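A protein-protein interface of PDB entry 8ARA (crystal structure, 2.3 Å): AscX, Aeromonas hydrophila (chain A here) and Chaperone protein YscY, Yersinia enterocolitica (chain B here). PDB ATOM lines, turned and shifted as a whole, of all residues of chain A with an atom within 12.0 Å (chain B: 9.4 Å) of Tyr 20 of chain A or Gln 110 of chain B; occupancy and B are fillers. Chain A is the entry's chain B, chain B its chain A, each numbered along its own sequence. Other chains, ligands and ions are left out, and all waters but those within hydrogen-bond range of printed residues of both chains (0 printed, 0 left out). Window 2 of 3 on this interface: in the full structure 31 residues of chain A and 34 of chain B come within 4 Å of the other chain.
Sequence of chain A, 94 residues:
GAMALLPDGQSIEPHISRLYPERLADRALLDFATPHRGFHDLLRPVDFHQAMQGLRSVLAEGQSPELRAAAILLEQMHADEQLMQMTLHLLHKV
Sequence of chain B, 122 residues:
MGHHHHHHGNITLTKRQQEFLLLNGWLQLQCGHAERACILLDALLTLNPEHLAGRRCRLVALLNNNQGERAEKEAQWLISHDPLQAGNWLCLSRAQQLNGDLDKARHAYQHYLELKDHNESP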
ATOM      1  N   ARG A  18     -27.017  27.491 -15.047  1.00  0.00           N
ATOM      2  CA  ARG A  18     -25.885  26.698 -15.513  1.00  0.00           C
ATOM      3  C   ARG A  18     -26.311  25.715 -16.614  1.00  0.00           C
ATOM      4  O   ARG A  18     -27.389  25.127 -16.550  1.00  0.00           O
ATOM      5  CB  ARG A  18     -25.240  25.955 -14.339  1.00  0.00           C
ATOM      6  CG  ARG A  18     -24.046  25.092 -14.724  1.00  0.00           C
ATOM      7  CD  ARG A  18     -23.092  24.895 -13.556  1.00  0.00           C
ATOM      8  NE  ARG A  18     -22.448  26.143 -13.163  1.00  0.00           N
ATOM      9  CZ  ARG A  18     -21.498  26.242 -12.242  1.00  0.00           C
ATOM     10  NH1 ARG A  18     -21.040  25.176 -11.603  1.00  0.00           N
ATOM     11  NH2 ARG A  18     -20.991  27.437 -11.958  1.00  0.00           N
ATOM     12  N   LEU A  19     -25.445  25.546 -17.619  1.00  0.00           N
ATOM     13  CA  LEU A  19     -25.798  24.761 -18.801  1.00  0.00           C
ATOM     14  C   LEU A  19     -26.001  23.292 -18.464  1.00  0.00           C
ATOM     15  O   LEU A  19     -26.976  22.670 -18.904  1.00  0.00           O
ATOM     16  CB  LEU A  19     -24.713  24.903 -19.867  1.00  0.00           C
ATOM     17  CG  LEU A  19     -24.684  26.189 -20.678  1.00  0.00           C
ATOM     18  CD1 LEU A  19     -23.429  26.228 -21.522  1.00  0.00           C
ATOM     19  CD2 LEU A  19     -25.924  26.269 -21.550  1.00  0.00           C
ATOM     20  N   TYR A  20     -25.076  22.711 -17.707  1.00  0.00           N
ATOM     21  CA  TYR A  20     -25.089  21.287 -17.450  1.00  0.00           C
ATOM     22  C   TYR A  20     -25.274  21.020 -15.963  1.00  0.00           C
ATOM     23  O   TYR A  20     -24.614  21.662 -15.133  1.00  0.00           O
ATOM     24  CB  TYR A  20     -23.789  20.639 -17.959  1.00  0.00           C
ATOM     25  CG  TYR A  20     -23.658  20.731 -19.464  1.00  0.00           C
ATOM     26  CD1 TYR A  20     -24.372  19.869 -20.290  1.00  0.00           C
ATOM     27  CD2 TYR A  20     -22.850  21.693 -20.061  1.00  0.00           C
ATOM     28  CE1 TYR A  20     -24.275  19.951 -21.668  1.00  0.00           C
ATOM     29  CE2 TYR A  20     -22.747  21.783 -21.443  1.00  0.00           C
ATOM     30  CZ  TYR A  20     -23.464  20.906 -22.240  1.00  0.00           C
ATOM     31  OH  TYR A  20     -23.378  20.977 -23.613  1.00  0.00           O
ATOM     32  N   PRO A  21     -26.176  20.089 -15.578  1.00  0.00           N
ATOM     33  CA  PRO A  21     -26.463  19.810 -14.166  1.00  0.00           C
ATOM     34  C   PRO A  21     -25.450  18.870 -13.513  1.00  0.00           C
ATOM     35  O   PRO A  21     -25.810  17.851 -12.927  1.00  0.00           O
ATOM     36  CB  PRO A  21     -27.855  19.176 -14.228  1.00  0.00           C
ATOM     37  CG  PRO A  21     -27.841  18.436 -15.531  1.00  0.00           C
ATOM     38  CD  PRO A  21     -27.005  19.265 -16.480  1.00  0.00           C
ATOM     39  N   GLU A  22     -24.167  19.217 -13.620  1.00  0.00           N
ATOM     40  CA  GLU A  22     -23.128  18.356 -13.067  1.00  0.00           C
ATOM     41  C   GLU A  22     -23.160  18.304 -11.546  1.00  0.00           C
ATOM     42  O   GLU A  22     -22.613  17.365 -10.963  1.00  0.00           O
ATOM     43  CB  GLU A  22     -21.751  18.819 -13.533  1.00  0.00           C
ATOM     44  CG  GLU A  22     -21.625  18.989 -15.030  1.00  0.00           C
ATOM     45  CD  GLU A  22     -20.184  19.098 -15.459  1.00  0.00           C
ATOM     46  OE1 GLU A  22     -19.404  18.180 -15.125  1.00  0.00           O
ATOM     47  OE2 GLU A  22     -19.825  20.104 -16.105  1.00  0.00           O
ATOM     48  N   ARG A  23     -23.783  19.289 -10.892  1.00  0.00           N
ATOM     49  CA  ARG A  23     -23.911  19.250  -9.440  1.00  0.00           C
ATOM     50  C   ARG A  23     -24.780  18.088  -8.975  1.00  0.00           C
ATOM     51  O   ARG A  23     -24.650  17.650  -7.829  1.00  0.00           O
ATOM     52  CB  ARG A  23     -24.475  20.580  -8.926  1.00  0.00           C
ATOM     53  CG  ARG A  23     -24.293  20.797  -7.423  1.00  0.00           C
ATOM     54  CD  ARG A  23     -24.737  22.190  -6.983  1.00  0.00           C
ATOM     55  NE  ARG A  23     -24.560  22.399  -5.549  1.00  0.00           N
ATOM     56  CZ  ARG A  23     -23.515  23.005  -4.998  1.00  0.00           C
ATOM     57  NH1 ARG A  23     -22.521  23.476  -5.733  1.00  0.00           N
ATOM     58  NH2 ARG A  23     -23.470  23.147  -3.675  1.00  0.00           N
ATOM     59  N   LEU A  24     -25.652  17.577  -9.842  1.00  0.00           N
ATOM     60  CA  LEU A  24     -26.507  16.437  -9.542  1.00  0.00           C
ATOM     61  C   LEU A  24     -25.918  15.113 -10.025  1.00  0.00           C
ATOM     62  O   LEU A  24     -26.580  14.077  -9.908  1.00  0.00           O
ATOM     63  CB  LEU A  24     -27.889  16.640 -10.173  1.00  0.00           C
ATOM     64  CG  LEU A  24     -28.638  17.930  -9.845  1.00  0.00           C
ATOM     65  CD1 LEU A  24     -29.957  17.979 -10.594  1.00  0.00           C
ATOM     66  CD2 LEU A  24     -28.864  18.058  -8.347  1.00  0.00           C
ATOM     67  N   ALA A  25     -24.698  15.129 -10.569  1.00  0.00           N
ATOM     68  CA  ALA A  25     -24.100  13.910 -11.103  1.00  0.00           C
ATOM     69  C   ALA A  25     -23.761  12.922  -9.996  1.00  0.00           C
ATOM     70  O   ALA A  25     -24.041  11.725 -10.121  1.00  0.00           O
ATOM     71  CB  ALA A  25     -22.849  14.248 -11.911  1.00  0.00           C
ATOM     72  N   ASP A  26     -23.144  13.398  -8.913  1.00  0.00           N
ATOM     73  CA  ASP A  26     -22.772  12.497  -7.829  1.00  0.00           C
ATOM     74  C   ASP A  26     -24.006  11.870  -7.196  1.00  0.00           C
ATOM     75  O   ASP A  26     -24.033  10.663  -6.936  1.00  0.00           O
ATOM     76  CB  ASP A  26     -21.949  13.243  -6.778  1.00  0.00           C
ATOM     77  CG  ASP A  26     -20.690  13.859  -7.351  1.00  0.00           C
ATOM     78  OD1 ASP A  26     -20.634  14.072  -8.582  1.00  0.00           O
ATOM     79  OD2 ASP A  26     -19.753  14.126  -6.569  1.00  0.00           O
ATOM     80  N   ALA A  28     -26.818  11.337  -8.614  1.00  0.00           N
ATOM     81  CA  ALA A  28     -27.418  10.401  -9.559  1.00  0.00           C
ATOM     82  C   ALA A  28     -26.649   9.087  -9.605  1.00  0.00           C
ATOM     83  O   ALA A  28     -27.246   8.021  -9.785  1.00  0.00           O
ATOM     84  CB  ALA A  28     -27.489  11.028 -10.949  1.00  0.00           C
ATOM     85  N   ALA B  86     -30.334   5.091 -18.561  1.00  0.00           N
ATOM     86  CA  ALA B  86     -29.484   6.247 -18.819  1.00  0.00           C
ATOM     87  C   ALA B  86     -28.287   6.296 -17.881  1.00  0.00           C
ATOM     88  O   ALA B  86     -27.228   6.808 -18.259  1.00  0.00           O
ATOM     89  CB  ALA B  86     -30.297   7.537 -18.700  1.00  0.00           C
ATOM     90  N   TRP B  89     -24.548   5.421 -19.077  1.00  0.00           N
ATOM     91  CA  TRP B  89     -23.672   6.360 -19.767  1.00  0.00           C
ATOM     92  C   TRP B  89     -23.083   7.386 -18.813  1.00  0.00           C
ATOM     93  O   TRP B  89     -21.998   7.920 -19.077  1.00  0.00           O
ATOM     94  CB  TRP B  89     -24.434   7.055 -20.889  1.00  0.00           C
ATOM     95  CG  TRP B  89     -24.892   6.115 -21.946  1.00  0.00           C
ATOM     96  CD1 TRP B  89     -26.078   5.445 -21.989  1.00  0.00           C
ATOM     97  CD2 TRP B  89     -24.168   5.727 -23.117  1.00  0.00           C
ATOM     98  NE1 TRP B  89     -26.141   4.666 -23.118  1.00  0.00           N
ATOM     99  CE2 TRP B  89     -24.981   4.821 -23.829  1.00  0.00           C
ATOM    100  CE3 TRP B  89     -22.913   6.058 -23.635  1.00  0.00           C
ATOM    101  CZ2 TRP B  89     -24.580   4.244 -25.031  1.00  0.00           C
ATOM    102  CZ3 TRP B  89     -22.519   5.483 -24.830  1.00  0.00           C
ATOM    103  CH2 TRP B  89     -23.348   4.587 -25.513  1.00  0.00           C
ATOM    104  N   LEU B  90     -23.786   7.687 -17.717  1.00  0.00           N
ATOM    105  CA  LEU B  90     -23.214   8.543 -16.685  1.00  0.00           C
ATOM    106  C   LEU B  90     -22.016   7.872 -16.030  1.00  0.00           C
ATOM    107  O   LEU B  90     -21.019   8.532 -15.720  1.00  0.00           O
ATOM    108  CB  LEU B  90     -24.273   8.892 -15.639  1.00  0.00           C
ATOM    109  CG  LEU B  90     -23.863   9.913 -14.569  1.00  0.00           C
ATOM    110  CD1 LEU B  90     -23.490  11.239 -15.210  1.00  0.00           C
ATOM    111  CD2 LEU B  90     -24.953  10.117 -13.521  1.00  0.00           C
ATOM    112  N   LEU B  92     -20.099   5.523 -17.538  1.00  0.00           N
ATOM    113  CA  LEU B  92     -19.059   5.552 -18.560  1.00  0.00           C
ATOM    114  C   LEU B  92     -18.417   6.929 -18.646  1.00  0.00           C
ATOM    115  O   LEU B  92     -17.203   7.046 -18.849  1.00  0.00           O
ATOM    116  CB  LEU B  92     -19.645   5.148 -19.912  1.00  0.00           C
ATOM    117  CG  LEU B  92     -18.674   5.099 -21.093  1.00  0.00           C
ATOM    118  CD1 LEU B  92     -17.693   3.945 -20.930  1.00  0.00           C
ATOM    119  CD2 LEU B  92     -19.430   4.990 -22.403  1.00  0.00           C
ATOM    120  N   SER B  93     -19.218   7.984 -18.487  1.00  0.00           N
ATOM    121  CA  SER B  93     -18.673   9.336 -18.500  1.00  0.00           C
ATOM    122  C   SER B  93     -17.672   9.540 -17.370  1.00  0.00           C
ATOM    123  O   SER B  93     -16.584  10.089 -17.582  1.00  0.00           O
ATOM    124  CB  SER B  93     -19.807  10.355 -18.399  1.00  0.00           C
ATOM    125  OG  SER B  93     -19.293  11.671 -18.357  1.00  0.00           O
ATOM    126  N   GLN B  96     -14.389   7.328 -18.020  1.00  0.00           N
ATOM    127  CA  GLN B  96     -13.539   7.929 -19.038  1.00  0.00           C
ATOM    128  C   GLN B  96     -12.945   9.243 -18.553  1.00  0.00           C
ATOM    129  O   GLN B  96     -11.855   9.629 -18.987  1.00  0.00           O
ATOM    130  CB  GLN B  96     -14.335   8.125 -20.327  1.00  0.00           C
ATOM    131  CG  GLN B  96     -14.746   6.810 -20.973  1.00  0.00           C
ATOM    132  CD  GLN B  96     -15.745   6.987 -22.098  1.00  0.00           C
ATOM    133  OE1 GLN B  96     -16.372   8.037 -22.233  1.00  0.00           O
ATOM    134  NE2 GLN B  96     -15.901   5.953 -22.912  1.00  0.00           N
ATOM    135  N   LEU B 102     -11.128  13.177 -21.700  1.00  0.00           N
ATOM    136  CA  LEU B 102     -12.221  14.111 -21.452  1.00  0.00           C
ATOM    137  C   LEU B 102     -13.163  14.211 -22.645  1.00  0.00           C
ATOM    138  O   LEU B 102     -14.356  14.480 -22.466  1.00  0.00           O
ATOM    139  CB  LEU B 102     -11.662  15.487 -21.101  1.00  0.00           C
ATOM    140  CG  LEU B 102     -12.673  16.478 -20.530  1.00  0.00           C
ATOM    141  CD1 LEU B 102     -13.193  15.982 -19.194  1.00  0.00           C
ATOM    142  CD2 LEU B 102     -12.052  17.858 -20.392  1.00  0.00           C
ATOM    143  N   ASP B 103     -12.654  14.001 -23.861  1.00  0.00           N
ATOM    144  CA  ASP B 103     -13.513  14.042 -25.041  1.00  0.00           C
ATOM    145  C   ASP B 103     -14.563  12.939 -24.991  1.00  0.00           C
ATOM    146  O   ASP B 103     -15.756  13.189 -25.201  1.00  0.00           O
ATOM    147  CB  ASP B 103     -12.670  13.921 -26.311  1.00  0.00           C
ATOM    148  CG  ASP B 103     -11.869  15.176 -26.605  1.00  0.00           C
ATOM    149  OD1 ASP B 103     -12.000  16.167 -25.850  1.00  0.00           O
ATOM    150  OD2 ASP B 103     -11.110  15.167 -27.599  1.00  0.00           O
ATOM    151  N   LYS B 104     -14.131  11.704 -24.725  1.00  0.00           N
ATOM    152  CA  LYS B 104     -15.080  10.605 -24.590  1.00  0.00           C
ATOM    153  C   LYS B 104     -16.043  10.846 -23.433  1.00  0.00           C
ATOM    154  O   LYS B 104     -17.249  10.600 -23.558  1.00  0.00           O
ATOM    155  CB  LYS B 104     -14.332   9.287 -24.389  1.00  0.00           C
ATOM    156  CG  LYS B 104     -13.500   8.828 -25.575  1.00  0.00           C
ATOM    157  CD  LYS B 104     -12.851   7.487 -25.268  1.00  0.00           C
ATOM    158  CE  LYS B 104     -12.107   6.930 -26.466  1.00  0.00           C
ATOM    159  NZ  LYS B 104     -11.489   5.612 -26.145  1.00  0.00           N
ATOM    160  N   ALA B 105     -15.527  11.326 -22.297  1.00  0.00           N
ATOM    161  CA  ALA B 105     -16.377  11.559 -21.135  1.00  0.00           C
ATOM    162  C   ALA B 105     -17.469  12.574 -21.435  1.00  0.00           C
ATOM    163  O   ALA B 105     -18.583  12.461 -20.912  1.00  0.00           O
ATOM    164  CB  ALA B 105     -15.532  12.023 -19.949  1.00  0.00           C
ATOM    165  N   ARG B 106     -17.174  13.563 -22.277  1.00  0.00           N
ATOM    166  CA  ARG B 106     -18.185  14.549 -22.643  1.00  0.00           C
ATOM    167  C   ARG B 106     -19.234  13.947 -23.567  1.00  0.00           C
ATOM    168  O   ARG B 106     -20.425  14.256 -23.445  1.00  0.00           O
ATOM    169  CB  ARG B 106     -17.520  15.758 -23.295  1.00  0.00           C
ATOM    170  CG  ARG B 106     -16.745  16.615 -22.323  1.00  0.00           C
ATOM    171  CD  ARG B 106     -16.027  17.740 -23.032  1.00  0.00           C
ATOM    172  NE  ARG B 106     -15.493  18.704 -22.078  1.00  0.00           N
ATOM    173  CZ  ARG B 106     -14.570  19.609 -22.365  1.00  0.00           C
ATOM    174  NH1 ARG B 106     -14.046  19.699 -23.577  1.00  0.00           N
ATOM    175  NH2 ARG B 106     -14.160  20.440 -21.412  1.00  0.00           N
ATOM    176  N   HIS B 107     -18.811  13.087 -24.500  1.00  0.00           N
ATOM    177  CA  HIS B 107     -19.763  12.443 -25.399  1.00  0.00           C
ATOM    178  C   HIS B 107     -20.681  11.493 -24.639  1.00  0.00           C
ATOM    179  O   HIS B 107     -21.892  11.456 -24.892  1.00  0.00           O
ATOM    180  CB  HIS B 107     -19.020  11.700 -26.510  1.00  0.00           C
ATOM    181  CG  HIS B 107     -19.910  11.193 -27.605  1.00  0.00           C
ATOM    182  ND1 HIS B 107     -20.009   9.856 -27.929  1.00  0.00           N
ATOM    183  CD2 HIS B 107     -20.740  11.846 -28.455  1.00  0.00           C
ATOM    184  CE1 HIS B 107     -20.861   9.707 -28.928  1.00  0.00           C
ATOM    185  NE2 HIS B 107     -21.319  10.899 -29.266  1.00  0.00           N
ATOM    186  N   ALA B 108     -20.124  10.719 -23.705  1.00  0.00           N
ATOM    187  CA  ALA B 108     -20.954   9.818 -22.915  1.00  0.00           C
ATOM    188  C   ALA B 108     -21.916  10.588 -22.020  1.00  0.00           C
ATOM    189  O   ALA B 108     -23.009  10.095 -21.720  1.00  0.00           O
ATOM    190  CB  ALA B 108     -20.075   8.885 -22.083  1.00  0.00           C
ATOM    191  N   TYR B 109     -21.536  11.795 -21.592  1.00  0.00           N
ATOM    192  CA  TYR B 109     -22.440  12.601 -20.778  1.00  0.00           C
ATOM    193  C   TYR B 109     -23.608  13.128 -21.599  1.00  0.00           C
ATOM    194  O   TYR B 109     -24.719  13.265 -21.073  1.00  0.00           O
ATOM    195  CB  TYR B 109     -21.679  13.758 -20.131  1.00  0.00           C
ATOM    196  CG  TYR B 109     -22.469  14.491 -19.071  1.00  0.00           C
ATOM    197  CD1 TYR B 109     -22.695  13.913 -17.829  1.00  0.00           C
ATOM    198  CD2 TYR B 109     -22.986  15.759 -19.308  1.00  0.00           C
ATOM    199  CE1 TYR B 109     -23.421  14.573 -16.853  1.00  0.00           C
ATOM    200  CE2 TYR B 109     -23.713  16.429 -18.334  1.00  0.00           C
ATOM    201  CZ  TYR B 109     -23.925  15.827 -17.109  1.00  0.00           C
ATOM    202  OH  TYR B 109     -24.643  16.473 -16.126  1.00  0.00           O
ATOM    203  N   GLN B 110     -23.379  13.427 -22.881  1.00  0.00           N
ATOM    204  CA  GLN B 110     -24.461  13.902 -23.737  1.00  0.00           C
ATOM    205  C   GLN B 110     -25.527  12.828 -23.910  1.00  0.00           C
ATOM    206  O   GLN B 110     -26.727  13.102 -23.791  1.00  0.00           O
ATOM    207  CB  GLN B 110     -23.913  14.333 -25.097  1.00  0.00           C
ATOM    208  CG  GLN B 110     -22.851  15.410 -25.022  1.00  0.00           C
ATOM    209  CD  GLN B 110     -23.304  16.625 -24.237  1.00  0.00           C
ATOM    210  OE1 GLN B 110     -24.424  17.108 -24.410  1.00  0.00           O
ATOM    211  NE2 GLN B 110     -22.434  17.122 -23.363  1.00  0.00           N
ATOM    212  N   HIS B 111     -25.102  11.594 -24.194  1.00  0.00           N
ATOM    213  CA  HIS B 111     -26.053  10.494 -24.300  1.00  0.00           C
ATOM    214  C   HIS B 111     -26.791  10.266 -22.985  1.00  0.00           C
ATOM    215  O   HIS B 111     -27.956   9.855 -22.992  1.00  0.00           O
ATOM    216  CB  HIS B 111     -25.336   9.218 -24.747  1.00  0.00           C
ATOM    217  CG  HIS B 111     -24.945   9.217 -26.194  1.00  0.00           C
ATOM    218  ND1 HIS B 111     -24.596   8.067 -26.870  1.00  0.00           N
ATOM    219  CD2 HIS B 111     -24.851  10.224 -27.094  1.00  0.00           C
ATOM    220  CE1 HIS B 111     -24.301   8.366 -28.122  1.00  0.00           C
ATOM    221  NE2 HIS B 111     -24.448   9.668 -28.286  1.00  0.00           N
ATOM    222  N   TYR B 112     -26.143  10.535 -21.852  1.00  0.00           N
ATOM    223  CA  TYR B 112     -26.849  10.465 -20.578  1.00  0.00           C
ATOM    224  C   TYR B 112     -27.967  11.500 -20.514  1.00  0.00           C
ATOM    225  O   TYR B 112     -29.079  11.199 -20.064  1.00  0.00           O
ATOM    226  CB  TYR B 112     -25.867  10.656 -19.422  1.00  0.00           C
ATOM    227  CG  TYR B 112     -26.525  11.026 -18.108  1.00  0.00           C
ATOM    228  CD1 TYR B 112     -27.174  10.070 -17.336  1.00  0.00           C
ATOM    229  CD2 TYR B 112     -26.489  12.332 -17.640  1.00  0.00           C
ATOM    230  CE1 TYR B 112     -27.777  10.415 -16.136  1.00  0.00           C
ATOM    231  CE2 TYR B 112     -27.082  12.683 -16.450  1.00  0.00           C
ATOM    232  CZ  TYR B 112     -27.724  11.726 -15.702  1.00  0.00           C
ATOM    233  OH  TYR B 112     -28.313  12.088 -14.514  1.00  0.00           O
ATOM    234  N   LEU B 113     -27.692  12.725 -20.965  1.00  0.00           N
ATOM    235  CA  LEU B 113     -28.715  13.763 -20.947  1.00  0.00           C
ATOM    236  C   LEU B 113     -29.836  13.451 -21.931  1.00  0.00           C
ATOM    237  O   LEU B 113     -31.015  13.674 -21.629  1.00  0.00           O
ATOM    238  CB  LEU B 113     -28.087  15.118 -21.262  1.00  0.00           C
ATOM    239  CG  LEU B 113     -27.019  15.597 -20.284  1.00  0.00           C
ATOM    240  CD1 LEU B 113     -26.518  16.974 -20.682  1.00  0.00           C
ATOM    241  CD2 LEU B 113     -27.559  15.604 -18.862  1.00  0.00           C
ATOM    242  N   GLU B 114     -29.487  12.940 -23.112  1.00  0.00           N
ATOM    243  CA  GLU B 114     -30.500  12.609 -24.108  1.00  0.00           C
ATOM    244  C   GLU B 114     -31.396  11.475 -23.627  1.00  0.00           C
ATOM    245  O   GLU B 114     -32.626  11.564 -23.709  1.00  0.00           O
ATOM    246  CB  GLU B 114     -29.826  12.241 -25.429  1.00  0.00           C
ATOM    247  CG  GLU B 114     -28.981  13.357 -26.013  1.00  0.00           C
ATOM    248  CD  GLU B 114     -28.195  12.917 -27.228  1.00  0.00           C
ATOM    249  OE1 GLU B 114     -28.255  11.716 -27.566  1.00  0.00           O
ATOM    250  OE2 GLU B 114     -27.518  13.770 -27.843  1.00  0.00           O
ATOM    251  N   LEU B 115     -30.795  10.398 -23.117  1.00  0.00           N
ATOM    252  CA  LEU B 115     -31.573   9.236 -22.705  1.00  0.00           C
ATOM    253  C   LEU B 115     -32.454   9.525 -21.495  1.00  0.00           C
ATOM    254  O   LEU B 115     -33.450   8.822 -21.292  1.00  0.00           O
ATOM    255  CB  LEU B 115     -30.640   8.060 -22.416  1.00  0.00           C
ATOM    256  CG  LEU B 115     -31.270   6.667 -22.445  1.00  0.00           C
ATOM    257  CD1 LEU B 115     -32.052   6.463 -23.735  1.00  0.00           C
ATOM    258  CD2 LEU B 115     -30.205   5.593 -22.296  1.00  0.00           C
ATOM    259  N   LYS B 116     -32.119  10.545 -20.697  1.00  0.00           N
ATOM    260  CA  LYS B 116     -32.980  10.916 -19.578  1.00  0.00           C
ATOM    261  C   LYS B 116     -34.310  11.486 -20.049  1.00  0.00           C
ATOM    262  O   LYS B 116     -35.328  11.321 -19.367  1.00  0.00           O
ATOM    263  CB  LYS B 116     -32.279  11.929 -18.679  1.00  0.00           C
ATOM    264  CG  LYS B 116     -31.310  11.317 -17.695  1.00  0.00           C
ATOM    265  CD  LYS B 116     -31.166  12.205 -16.478  1.00  0.00           C
ATOM    266  CE  LYS B 116     -32.510  12.411 -15.804  1.00  0.00           C
ATOM    267  NZ  LYS B 116     -32.377  13.200 -14.551  1.00  0.00           N
ATOM    268  N   ASP B 117     -34.322  12.161 -21.197  1.00  0.00           N
ATOM    269  CA  ASP B 117     -35.540  12.759 -21.732  1.00  0.00           C
ATOM    270  C   ASP B 117     -36.364  11.791 -22.572  1.00  0.00           C
ATOM    271  O   ASP B 117     -37.510  12.113 -22.904  1.00  0.00           O
ATOM    272  CB  ASP B 117     -35.194  13.997 -22.565  1.00  0.00           C
ATOM    273  CG  ASP B 117     -34.292  14.965 -21.820  1.00  0.00           C
ATOM    274  OD1 ASP B 117     -33.913  14.668 -20.666  1.00  0.00           O
ATOM    275  OD2 ASP B 117     -33.958  16.025 -22.393  1.00  0.00           O
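Tyr 20 of chain A touches Gln 110 of chain B (CE1 to NE2, 3.8 Å). CD1 of Leu 113 of chain B touches CD1 of Tyr 20 of chain A, 3.6 Å away. Pro 21 of chain A touches Tyr 109 of chain B. Glu 22 of chain A touches Tyr 109 of chain B (N to OH, 3.7 Å). Leu 90 of chain B touches Ala 25 of chain A (CD2 to O, 3.9 Å). CB of Ala 28 of chain A touches CD2 of Leu 90 of chain B, 3.7 Å away. Ala 28 of chain A touches Tyr 112 of chain B (CB to OH, 3.8 Å).
Of the printed residues of chain B, Tyr 20 of chain A touches Gln 110 and Leu 113. Of chain A, only Tyr 20 (3.8 Å) comes within 4 Å of Gln 110 of chain B. No residue of chain B comes within 4 Å of Leu 19 of chain A. No residue of chain A comes within 4 Å of His 107 of chain B. No residue of chain A comes within 4 Å of His 111 of chain B. Leu 113 of chain B touches one residue of chain A. No residue of chain A comes within 4 Å of Glu 114 of chain B. Printed residues of chain A within 4 Å of Tyr 112 of chain B: Ala 28 (3.8 Å). Of the printed residues of chain B, Ala 28 of chain A touches Leu 90 (3.7 Å) and Tyr 112 (3.8 Å). Of the printed residues of chain A, Tyr 109 of chain B touches Pro 21 (3.6 Å) and Glu 22 (3.7 Å). The nearest printed residue of chain B that does not touch Tyr 20 of chain A is Tyr 109 of chain B (4.01 Å).
Of the 22 printed residues of chain B, 5 touch a printed residue of chain A. Printed residues of chain A that touch a printed residue of chain B: Tyr 20, Pro 21, Glu 22, Ala 25 and Ala 28.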
